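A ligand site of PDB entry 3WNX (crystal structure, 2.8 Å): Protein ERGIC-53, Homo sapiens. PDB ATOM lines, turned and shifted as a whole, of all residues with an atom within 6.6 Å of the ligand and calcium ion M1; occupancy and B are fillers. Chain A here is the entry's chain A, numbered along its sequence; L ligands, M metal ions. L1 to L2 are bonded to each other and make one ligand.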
ATOM      1  N   LYS A  64     -10.593   7.688  32.072  1.00  0.00           N
ATOM      2  CA  LYS A  64      -9.434   6.824  32.091  1.00  0.00           C
ATOM      3  C   LYS A  64      -9.845   5.372  31.989  1.00  0.00           C
ATOM      4  O   LYS A  64     -10.585   4.876  32.845  1.00  0.00           O
ATOM      5  CB  LYS A  64      -8.636   6.987  33.382  1.00  0.00           C
ATOM      6  CG  LYS A  64      -7.480   7.976  33.297  1.00  0.00           C
ATOM      7  CD  LYS A  64      -6.749   8.035  34.629  1.00  0.00           C
ATOM      8  CE  LYS A  64      -6.291   9.444  34.977  1.00  0.00           C
ATOM      9  NZ  LYS A  64      -5.094   9.870  34.196  1.00  0.00           N
ATOM     10  N   SER A  65      -9.333   4.700  30.964  1.00  0.00           N
ATOM     11  CA  SER A  65      -9.391   3.243  30.879  1.00  0.00           C
ATOM     12  C   SER A  65     -10.820   2.752  30.734  1.00  0.00           C
ATOM     13  O   SER A  65     -11.296   1.934  31.505  1.00  0.00           O
ATOM     14  CB  SER A  65      -8.704   2.598  32.091  1.00  0.00           C
ATOM     15  OG  SER A  65      -7.464   3.221  32.358  1.00  0.00           O
ATOM     16  N   GLN A  66     -11.496   3.264  29.705  1.00  0.00           N
ATOM     17  CA  GLN A  66     -12.856   2.867  29.438  1.00  0.00           C
ATOM     18  C   GLN A  66     -12.891   1.754  28.430  1.00  0.00           C
ATOM     19  O   GLN A  66     -12.003   1.612  27.595  1.00  0.00           O
ATOM     20  CB  GLN A  66     -13.664   4.075  28.938  1.00  0.00           C
ATOM     21  CG  GLN A  66     -13.902   5.097  30.028  1.00  0.00           C
ATOM     22  CD  GLN A  66     -14.533   4.436  31.231  1.00  0.00           C
ATOM     23  OE1 GLN A  66     -15.531   3.752  31.088  1.00  0.00           O
ATOM     24  NE2 GLN A  66     -13.943   4.607  32.397  1.00  0.00           N
ATOM     25  N   ARG A  67     -13.947   0.951  28.540  1.00  0.00           N
ATOM     26  CA  ARG A  67     -14.245  -0.081  27.583  1.00  0.00           C
ATOM     27  C   ARG A  67     -15.748  -0.107  27.495  1.00  0.00           C
ATOM     28  O   ARG A  67     -16.414  -0.205  28.518  1.00  0.00           O
ATOM     29  CB  ARG A  67     -13.762  -1.453  28.066  1.00  0.00           C
ATOM     30  CG  ARG A  67     -12.263  -1.669  27.931  1.00  0.00           C
ATOM     31  CD  ARG A  67     -11.947  -3.146  28.121  1.00  0.00           C
ATOM     32  NE  ARG A  67     -10.514  -3.410  28.288  1.00  0.00           N
ATOM     33  CZ  ARG A  67      -9.993  -4.457  28.914  1.00  0.00           C
ATOM     34  NH1 ARG A  67     -10.788  -5.390  29.442  1.00  0.00           N
ATOM     35  NH2 ARG A  67      -8.677  -4.570  29.013  1.00  0.00           N
ATOM     36  N   GLY A  96      -5.312  12.081  21.098  1.00  0.00           N
ATOM     37  CA  GLY A  96      -6.404  11.421  21.813  1.00  0.00           C
ATOM     38  C   GLY A  96      -6.297   9.904  21.760  1.00  0.00           C
ATOM     39  O   GLY A  96      -5.384   9.350  21.144  1.00  0.00           O
ATOM     40  N   ALA A  97      -7.237   9.221  22.401  1.00  0.00           N
ATOM     41  CA  ALA A  97      -7.152   7.757  22.509  1.00  0.00           C
ATOM     42  C   ALA A  97      -8.472   7.165  22.961  1.00  0.00           C
ATOM     43  O   ALA A  97      -9.338   7.909  23.424  1.00  0.00           O
ATOM     44  CB  ALA A  97      -6.050   7.383  23.497  1.00  0.00           C
ATOM     45  N   ASP A  98      -8.655   5.847  22.828  1.00  0.00           N
ATOM     46  CA  ASP A  98      -7.753   4.974  22.058  1.00  0.00           C
ATOM     47  C   ASP A  98      -8.261   4.750  20.655  1.00  0.00           C
ATOM     48  O   ASP A  98      -7.479   4.571  19.713  1.00  0.00           O
ATOM     49  CB  ASP A  98      -7.575   3.612  22.743  1.00  0.00           C
ATOM     50  CG  ASP A  98      -6.311   3.542  23.563  1.00  0.00           C
ATOM     51  OD1 ASP A  98      -6.350   2.945  24.665  1.00  0.00           O
ATOM     52  OD2 ASP A  98      -5.279   4.092  23.090  1.00  0.00           O
ATOM     53  N   PHE A 115     -10.219  -2.710  21.726  1.00  0.00           N
ATOM     54  CA  PHE A 115     -11.099  -1.539  21.637  1.00  0.00           C
ATOM     55  C   PHE A 115     -12.414  -1.762  22.390  1.00  0.00           C
ATOM     56  O   PHE A 115     -13.487  -1.517  21.858  1.00  0.00           O
ATOM     57  CB  PHE A 115     -11.342  -1.198  20.166  1.00  0.00           C
ATOM     58  CG  PHE A 115     -10.118  -0.735  19.454  1.00  0.00           C
ATOM     59  CD1 PHE A 115      -9.937   0.609  19.173  1.00  0.00           C
ATOM     60  CD2 PHE A 115      -9.121  -1.629  19.074  1.00  0.00           C
ATOM     61  CE1 PHE A 115      -8.794   1.057  18.527  1.00  0.00           C
ATOM     62  CE2 PHE A 115      -7.982  -1.190  18.432  1.00  0.00           C
ATOM     63  CZ  PHE A 115      -7.825   0.156  18.157  1.00  0.00           C
ATOM     64  N   ASP A 129      -7.995   3.878  14.855  1.00  0.00           N
ATOM     65  CA  ASP A 129      -6.936   3.987  15.863  1.00  0.00           C
ATOM     66  C   ASP A 129      -6.502   5.427  16.023  1.00  0.00           C
ATOM     67  O   ASP A 129      -5.747   5.955  15.208  1.00  0.00           O
ATOM     68  CB  ASP A 129      -5.750   3.109  15.468  1.00  0.00           C
ATOM     69  CG  ASP A 129      -4.782   2.829  16.609  1.00  0.00           C
ATOM     70  OD1 ASP A 129      -4.497   3.742  17.431  1.00  0.00           O
ATOM     71  OD2 ASP A 129      -4.292   1.677  16.699  1.00  0.00           O
ATOM     72  N   SER A 130      -7.003   6.081  17.078  1.00  0.00           N
ATOM     73  CA  SER A 130      -6.617   7.454  17.395  1.00  0.00           C
ATOM     74  C   SER A 130      -5.154   7.503  17.817  1.00  0.00           C
ATOM     75  O   SER A 130      -4.442   8.446  17.476  1.00  0.00           O
ATOM     76  CB  SER A 130      -7.457   8.033  18.550  1.00  0.00           C
ATOM     77  OG  SER A 130      -8.840   7.759  18.409  1.00  0.00           O
ATOM     78  N   PHE A 131      -4.736   6.492  18.582  1.00  0.00           N
ATOM     79  CA  PHE A 131      -3.441   6.563  19.261  1.00  0.00           C
ATOM     80  C   PHE A 131      -2.302   5.786  18.583  1.00  0.00           C
ATOM     81  O   PHE A 131      -2.351   4.555  18.391  1.00  0.00           O
ATOM     82  CB  PHE A 131      -3.564   6.130  20.723  1.00  0.00           C
ATOM     83  CG  PHE A 131      -2.340   6.468  21.532  1.00  0.00           C
ATOM     84  CD1 PHE A 131      -1.923   7.786  21.665  1.00  0.00           C
ATOM     85  CD2 PHE A 131      -1.581   5.461  22.143  1.00  0.00           C
ATOM     86  CE1 PHE A 131      -0.788   8.106  22.405  1.00  0.00           C
ATOM     87  CE2 PHE A 131      -0.445   5.766  22.881  1.00  0.00           C
ATOM     88  CZ  PHE A 131      -0.046   7.096  23.017  1.00  0.00           C
ATOM     89  N   ASP A 132      -1.261   6.560  18.263  1.00  0.00           N
ATOM     90  CA  ASP A 132      -0.050   6.101  17.609  1.00  0.00           C
ATOM     91  C   ASP A 132       0.776   5.122  18.490  1.00  0.00           C
ATOM     92  O   ASP A 132       1.846   5.488  18.998  1.00  0.00           O
ATOM     93  CB  ASP A 132       0.781   7.347  17.253  1.00  0.00           C
ATOM     94  CG  ASP A 132       1.971   7.040  16.385  1.00  0.00           C
ATOM     95  OD1 ASP A 132       1.863   6.140  15.520  1.00  0.00           O
ATOM     96  OD2 ASP A 132       3.008   7.713  16.549  1.00  0.00           O
ATOM     97  N   ASN A 133       0.298   3.889  18.643  1.00  0.00           N
ATOM     98  CA  ASN A 133       0.864   2.973  19.652  1.00  0.00           C
ATOM     99  C   ASN A 133       2.263   2.405  19.346  1.00  0.00           C
ATOM    100  O   ASN A 133       3.003   2.076  20.286  1.00  0.00           O
ATOM    101  CB  ASN A 133      -0.097   1.827  19.975  1.00  0.00           C
ATOM    102  CG  ASN A 133      -1.336   2.306  20.705  1.00  0.00           C
ATOM    103  OD1 ASN A 133      -2.178   3.013  20.132  1.00  0.00           O
ATOM    104  ND2 ASN A 133      -1.485   1.914  21.968  1.00  0.00           N
ATOM    105  N   ASP A 134       2.623   2.268  18.067  1.00  0.00           N
ATOM    106  CA  ASP A 134       3.987   1.843  17.689  1.00  0.00           C
ATOM    107  C   ASP A 134       4.900   3.049  17.394  1.00  0.00           C
ATOM    108  O   ASP A 134       5.908   2.918  16.707  1.00  0.00           O
ATOM    109  CB  ASP A 134       3.986   0.821  16.537  1.00  0.00           C
ATOM    110  CG  ASP A 134       2.974   1.139  15.434  1.00  0.00           C
ATOM    111  OD1 ASP A 134       2.909   2.313  15.016  1.00  0.00           O
ATOM    112  OD2 ASP A 134       2.263   0.221  14.981  1.00  0.00           O
ATOM    113  N   ASN A 139      -0.665   7.657  12.800  1.00  0.00           N
ATOM    114  CA  ASN A 139      -1.995   7.801  13.352  1.00  0.00           C
ATOM    115  C   ASN A 139      -2.486   9.242  13.268  1.00  0.00           C
ATOM    116  O   ASN A 139      -1.663  10.138  13.068  1.00  0.00           O
ATOM    117  CB  ASN A 139      -2.018   7.244  14.780  1.00  0.00           C
ATOM    118  CG  ASN A 139      -2.114   5.737  14.791  1.00  0.00           C
ATOM    119  OD1 ASN A 139      -1.721   5.073  13.839  1.00  0.00           O
ATOM    120  ND2 ASN A 139      -2.672   5.182  15.846  1.00  0.00           N
ATOM    121  N   TYR A 153      -4.799  -9.483  18.625  1.00  0.00           N
ATOM    122  CA  TYR A 153      -4.612  -8.174  18.000  1.00  0.00           C
ATOM    123  C   TYR A 153      -3.378  -7.495  18.573  1.00  0.00           C
ATOM    124  O   TYR A 153      -3.286  -7.279  19.789  1.00  0.00           O
ATOM    125  CB  TYR A 153      -5.846  -7.278  18.173  1.00  0.00           C
ATOM    126  CG  TYR A 153      -5.544  -5.814  17.989  1.00  0.00           C
ATOM    127  CD1 TYR A 153      -5.188  -5.314  16.751  1.00  0.00           C
ATOM    128  CD2 TYR A 153      -5.589  -4.932  19.059  1.00  0.00           C
ATOM    129  CE1 TYR A 153      -4.900  -3.970  16.576  1.00  0.00           C
ATOM    130  CE2 TYR A 153      -5.312  -3.586  18.907  1.00  0.00           C
ATOM    131  CZ  TYR A 153      -4.965  -3.107  17.662  1.00  0.00           C
ATOM    132  OH  TYR A 153      -4.665  -1.764  17.503  1.00  0.00           O
ATOM    133  N   HIS A 155      -2.013  -4.901  19.724  1.00  0.00           N
ATOM    134  CA  HIS A 155      -2.435  -3.583  20.192  1.00  0.00           C
ATOM    135  C   HIS A 155      -1.302  -2.566  20.088  1.00  0.00           C
ATOM    136  O   HIS A 155      -1.465  -1.527  19.449  1.00  0.00           O
ATOM    137  CB  HIS A 155      -2.962  -3.641  21.634  1.00  0.00           C
ATOM    138  CG  HIS A 155      -3.612  -2.370  22.083  1.00  0.00           C
ATOM    139  ND1 HIS A 155      -4.981  -2.199  22.121  1.00  0.00           N
ATOM    140  CD2 HIS A 155      -3.078  -1.202  22.520  1.00  0.00           C
ATOM    141  CE1 HIS A 155      -5.264  -0.985  22.563  1.00  0.00           C
ATOM    142  NE2 HIS A 155      -4.126  -0.353  22.812  1.00  0.00           N
ATOM    143  N   GLN A 156      -0.163  -2.898  20.694  1.00  0.00           N
ATOM    144  CA  GLN A 156       0.974  -1.974  20.779  1.00  0.00           C
ATOM    145  C   GLN A 156       1.505  -1.593  19.406  1.00  0.00           C
ATOM    146  O   GLN A 156       2.079  -0.512  19.261  1.00  0.00           O
ATOM    147  CB  GLN A 156       2.117  -2.545  21.626  1.00  0.00           C
ATOM    148  CG  GLN A 156       1.831  -2.654  23.125  1.00  0.00           C
ATOM    149  CD  GLN A 156       1.437  -4.062  23.570  1.00  0.00           C
ATOM    150  OE1 GLN A 156       0.864  -4.841  22.808  1.00  0.00           O
ATOM    151  NE2 GLN A 156       1.746  -4.390  24.829  1.00  0.00           N
ATOM    152  N   ASN A 157       1.318  -2.457  18.413  1.00  0.00           N
ATOM    153  CA  ASN A 157       1.734  -2.164  17.030  1.00  0.00           C
ATOM    154  C   ASN A 157       0.577  -1.786  16.101  1.00  0.00           C
ATOM    155  O   ASN A 157       0.670  -1.988  14.886  1.00  0.00           O
ATOM    156  CB  ASN A 157       2.516  -3.335  16.433  1.00  0.00           C
ATOM    157  CG  ASN A 157       3.871  -3.527  17.097  1.00  0.00           C
ATOM    158  OD1 ASN A 157       4.647  -2.571  17.223  1.00  0.00           O
ATOM    159  ND2 ASN A 157       4.167  -4.758  17.515  1.00  0.00           N
ATOM    160  N   ASP A 158      -0.496  -1.242  16.667  1.00  0.00           N
ATOM    161  CA  ASP A 158      -1.691  -0.918  15.912  1.00  0.00           C
ATOM    162  C   ASP A 158      -2.210  -2.089  15.072  1.00  0.00           C
ATOM    163  O   ASP A 158      -3.147  -1.911  14.308  1.00  0.00           O
ATOM    164  CB  ASP A 158      -1.434   0.262  14.965  1.00  0.00           C
ATOM    165  CG  ASP A 158      -0.830   1.461  15.657  1.00  0.00           C
ATOM    166  OD1 ASP A 158      -0.878   1.543  16.897  1.00  0.00           O
ATOM    167  OD2 ASP A 158      -0.302   2.331  14.933  1.00  0.00           O
ATOM    168  N   THR A 227     -10.503   3.662  25.993  1.00  0.00           N
ATOM    169  CA  THR A 227      -9.598   4.729  26.380  1.00  0.00           C
ATOM    170  C   THR A 227      -8.539   4.090  27.307  1.00  0.00           C
ATOM    171  O   THR A 227      -8.700   2.943  27.745  1.00  0.00           O
ATOM    172  CB  THR A 227     -10.365   5.892  27.094  1.00  0.00           C
ATOM    173  OG1 THR A 227     -10.968   5.427  28.317  1.00  0.00           O
ATOM    174  CG2 THR A 227     -11.482   6.466  26.200  1.00  0.00           C
ATOM    175  N   GLY A 228      -7.474   4.826  27.605  1.00  0.00           N
ATOM    176  CA  GLY A 228      -6.459   4.364  28.560  1.00  0.00           C
ATOM    177  C   GLY A 228      -5.963   5.461  29.483  1.00  0.00           C
ATOM    178  O   GLY A 228      -6.684   5.924  30.379  1.00  0.00           O
ATOM    179  N   GLY A 229      -4.721   5.876  29.263  1.00  0.00           N
ATOM    180  CA  GLY A 229      -4.162   7.030  29.964  1.00  0.00           C
ATOM    181  C   GLY A 229      -4.730   8.298  29.355  1.00  0.00           C
ATOM    182  O   GLY A 229      -5.019   9.263  30.058  1.00  0.00           O
ATOM    183  N   LEU A 230      -4.868   8.273  28.024  1.00  0.00           N
ATOM    184  CA  LEU A 230      -5.608   9.283  27.268  1.00  0.00           C
ATOM    185  C   LEU A 230      -6.989   8.756  26.886  1.00  0.00           C
ATOM    186  O   LEU A 230      -7.208   7.541  26.902  1.00  0.00           O
ATOM    187  CB  LEU A 230      -4.844   9.655  26.013  1.00  0.00           C
ATOM    188  CG  LEU A 230      -3.688  10.641  26.188  1.00  0.00           C
ATOM    189  CD1 LEU A 230      -2.803  10.601  24.954  1.00  0.00           C
ATOM    190  CD2 LEU A 230      -4.217  12.050  26.422  1.00  0.00           C
ATOM    191  N   ALA A 231      -7.908   9.664  26.537  1.00  0.00           N
ATOM    192  CA  ALA A 231      -9.346   9.337  26.402  1.00  0.00           C
ATOM    193  C   ALA A 231     -10.136  10.402  25.661  1.00  0.00           C
ATOM    194  O   ALA A 231     -10.156  11.544  26.078  1.00  0.00           O
ATOM    195  CB  ALA A 231      -9.971   9.171  27.779  1.00  0.00           C
HETATM  196  C1  LIG L   1      -1.247   4.310  27.871  1.00  0.00           C
HETATM  197  C2  LIG L   1      -1.494   2.803  27.631  1.00  0.00           C
HETATM  198  C3  LIG L   1      -1.712   2.400  26.178  1.00  0.00           C
HETATM  199  C4  LIG L   1      -2.678   3.366  25.531  1.00  0.00           C
HETATM  200  C5  LIG L   1      -2.263   4.813  25.772  1.00  0.00           C
HETATM  201  C6  LIG L   1      -3.316   5.790  25.250  1.00  0.00           C
HETATM  202  O1  LIG L   1       0.080   4.733  27.541  1.00  0.00           O
HETATM  203  O2  LIG L   1      -2.669   2.335  28.277  1.00  0.00           O
HETATM  204  O3  LIG L   1      -2.307   1.116  26.115  1.00  0.00           O
HETATM  205  O4  LIG L   1      -2.703   3.062  24.152  1.00  0.00           O
HETATM  206  O5  LIG L   1      -2.153   5.095  27.145  1.00  0.00           O
HETATM  207  O6  LIG L   1      -4.507   5.677  26.019  1.00  0.00           O
HETATM  208  C1  LG2 L   2      -2.398   1.160  29.070  1.00  0.00           C
HETATM  209  C2  LG2 L   2      -3.712   0.448  29.409  1.00  0.00           C
HETATM  210  C3  LG2 L   2      -4.531   1.325  30.383  1.00  0.00           C
HETATM  211  C4  LG2 L   2      -3.650   1.947  31.497  1.00  0.00           C
HETATM  212  C5  LG2 L   2      -2.388   2.586  30.912  1.00  0.00           C
HETATM  213  C6  LG2 L   2      -1.429   3.257  31.922  1.00  0.00           C
HETATM  214  O1  LG2 L   2      -3.483  -0.876  29.896  1.00  0.00           O
HETATM  215  O2  LG2 L   2      -5.657   0.658  30.919  1.00  0.00           O
HETATM  216  O3  LG2 L   2      -4.419   2.917  32.144  1.00  0.00           O
HETATM  217  O4  LG2 L   2      -1.713   1.533  30.238  1.00  0.00           O
HETATM  218  O5  LG2 L   2      -0.858   4.446  31.391  1.00  0.00           O
HETATM  219 CA    CA M   1      -3.436   2.144  18.729  1.00  0.00          CA
HETATM  220 CA    CA M   2       0.851   3.882  15.148  1.00  0.00          CA
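OD1 of Asn 133 is bound to calcium ion M1, 2.1 Å away.
OD2 of Asp 129 binds calcium ion M1, at 2.3 Å.
OD1 of Asp 129 is bound to calcium ion M1, 2.3 Å away.
Calcium ion M1 is bound by O of Phe 131 (2.7 Å).
Residues that only touch calcium ion M1: Asp 158 (3.2 Å).
Within 4 Å of calcium ion M1: Asp 129, Phe 131, Asn 133 and Asp 158.
The nearest printed residue that does not touch calcium ion M1 is His 155 (4.2 Å).
Residues that only touch the ligand: Ala 97 (3.4 Å) and His 155 (3.9 Å).
Hydrophobic or aromatic side chains within 4 Å of the ligand: Ala 97, Phe 131 and Leu 230.
Within 4 Å of the ligand: Ser 65, Ala 97, Asp 98, Phe 131, Asn 133, His 155, Gly 228, Gly 229 and Leu 230.
Along chain A the residues within 4 Å of the ligand span positions 65 to 230.
The side-chain carboxylate (OD2) of Asp 158 sits close to the side-chain amide oxygen (OD1) of Asn 139, at 3.3 Å.
The backbone NH of Ser 65 is in hydrogen-bond range of the backbone carbonyl oxygen of Gly 228, 3.0 Å away.
The side-chain amide nitrogen (ND2) of Asn 139 is in hydrogen-bond range of the backbone carbonyl oxygen (O) of Asp 129 (3.2 Å).
ND2 of Asn 139 lies close to O of Phe 131.
N of Asn 133 sits at hydrogen-bond distance from OD1 of Asp 158 (3.2 Å).
The backbone NH (N) of Ser 130 lies within hydrogen-bond range of the backbone carbonyl oxygen (O) of Asp 98, 3.1 Å away.
The backbone NH of Ser 65 lies within hydrogen-bond range of the side-chain hydroxyl of Thr 227, 3.2 Å away.
An oxygen (O6) of LIG L1 lies within hydrogen-bond range of the backbone NH (N) of Leu 230 (3.3 Å).
OD2 of Asp 98 lies within hydrogen-bond range of O4 of LIG L1 (3.0 Å).
The backbone carbonyl oxygen of Leu 230 is in hydrogen-bond range of an oxygen (O6) of LIG L1, 3.4 Å away.
N of Gly 229 lies within hydrogen-bond range of O6 of LIG L1, 3.3 Å away.
The side-chain amide nitrogen (ND2) of Asn 133 is in hydrogen-bond range of an oxygen (O4) of LIG L1 (2.8 Å).
The side-chain hydroxyl (OG) of Ser 65 sits at hydrogen-bond distance from an oxygen (O3) of LG2 L2, 3.1 Å away.
The backbone NH (N) of Gly 228 lies close to an oxygen (O6) of LIG L1, 3.5 Å away.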
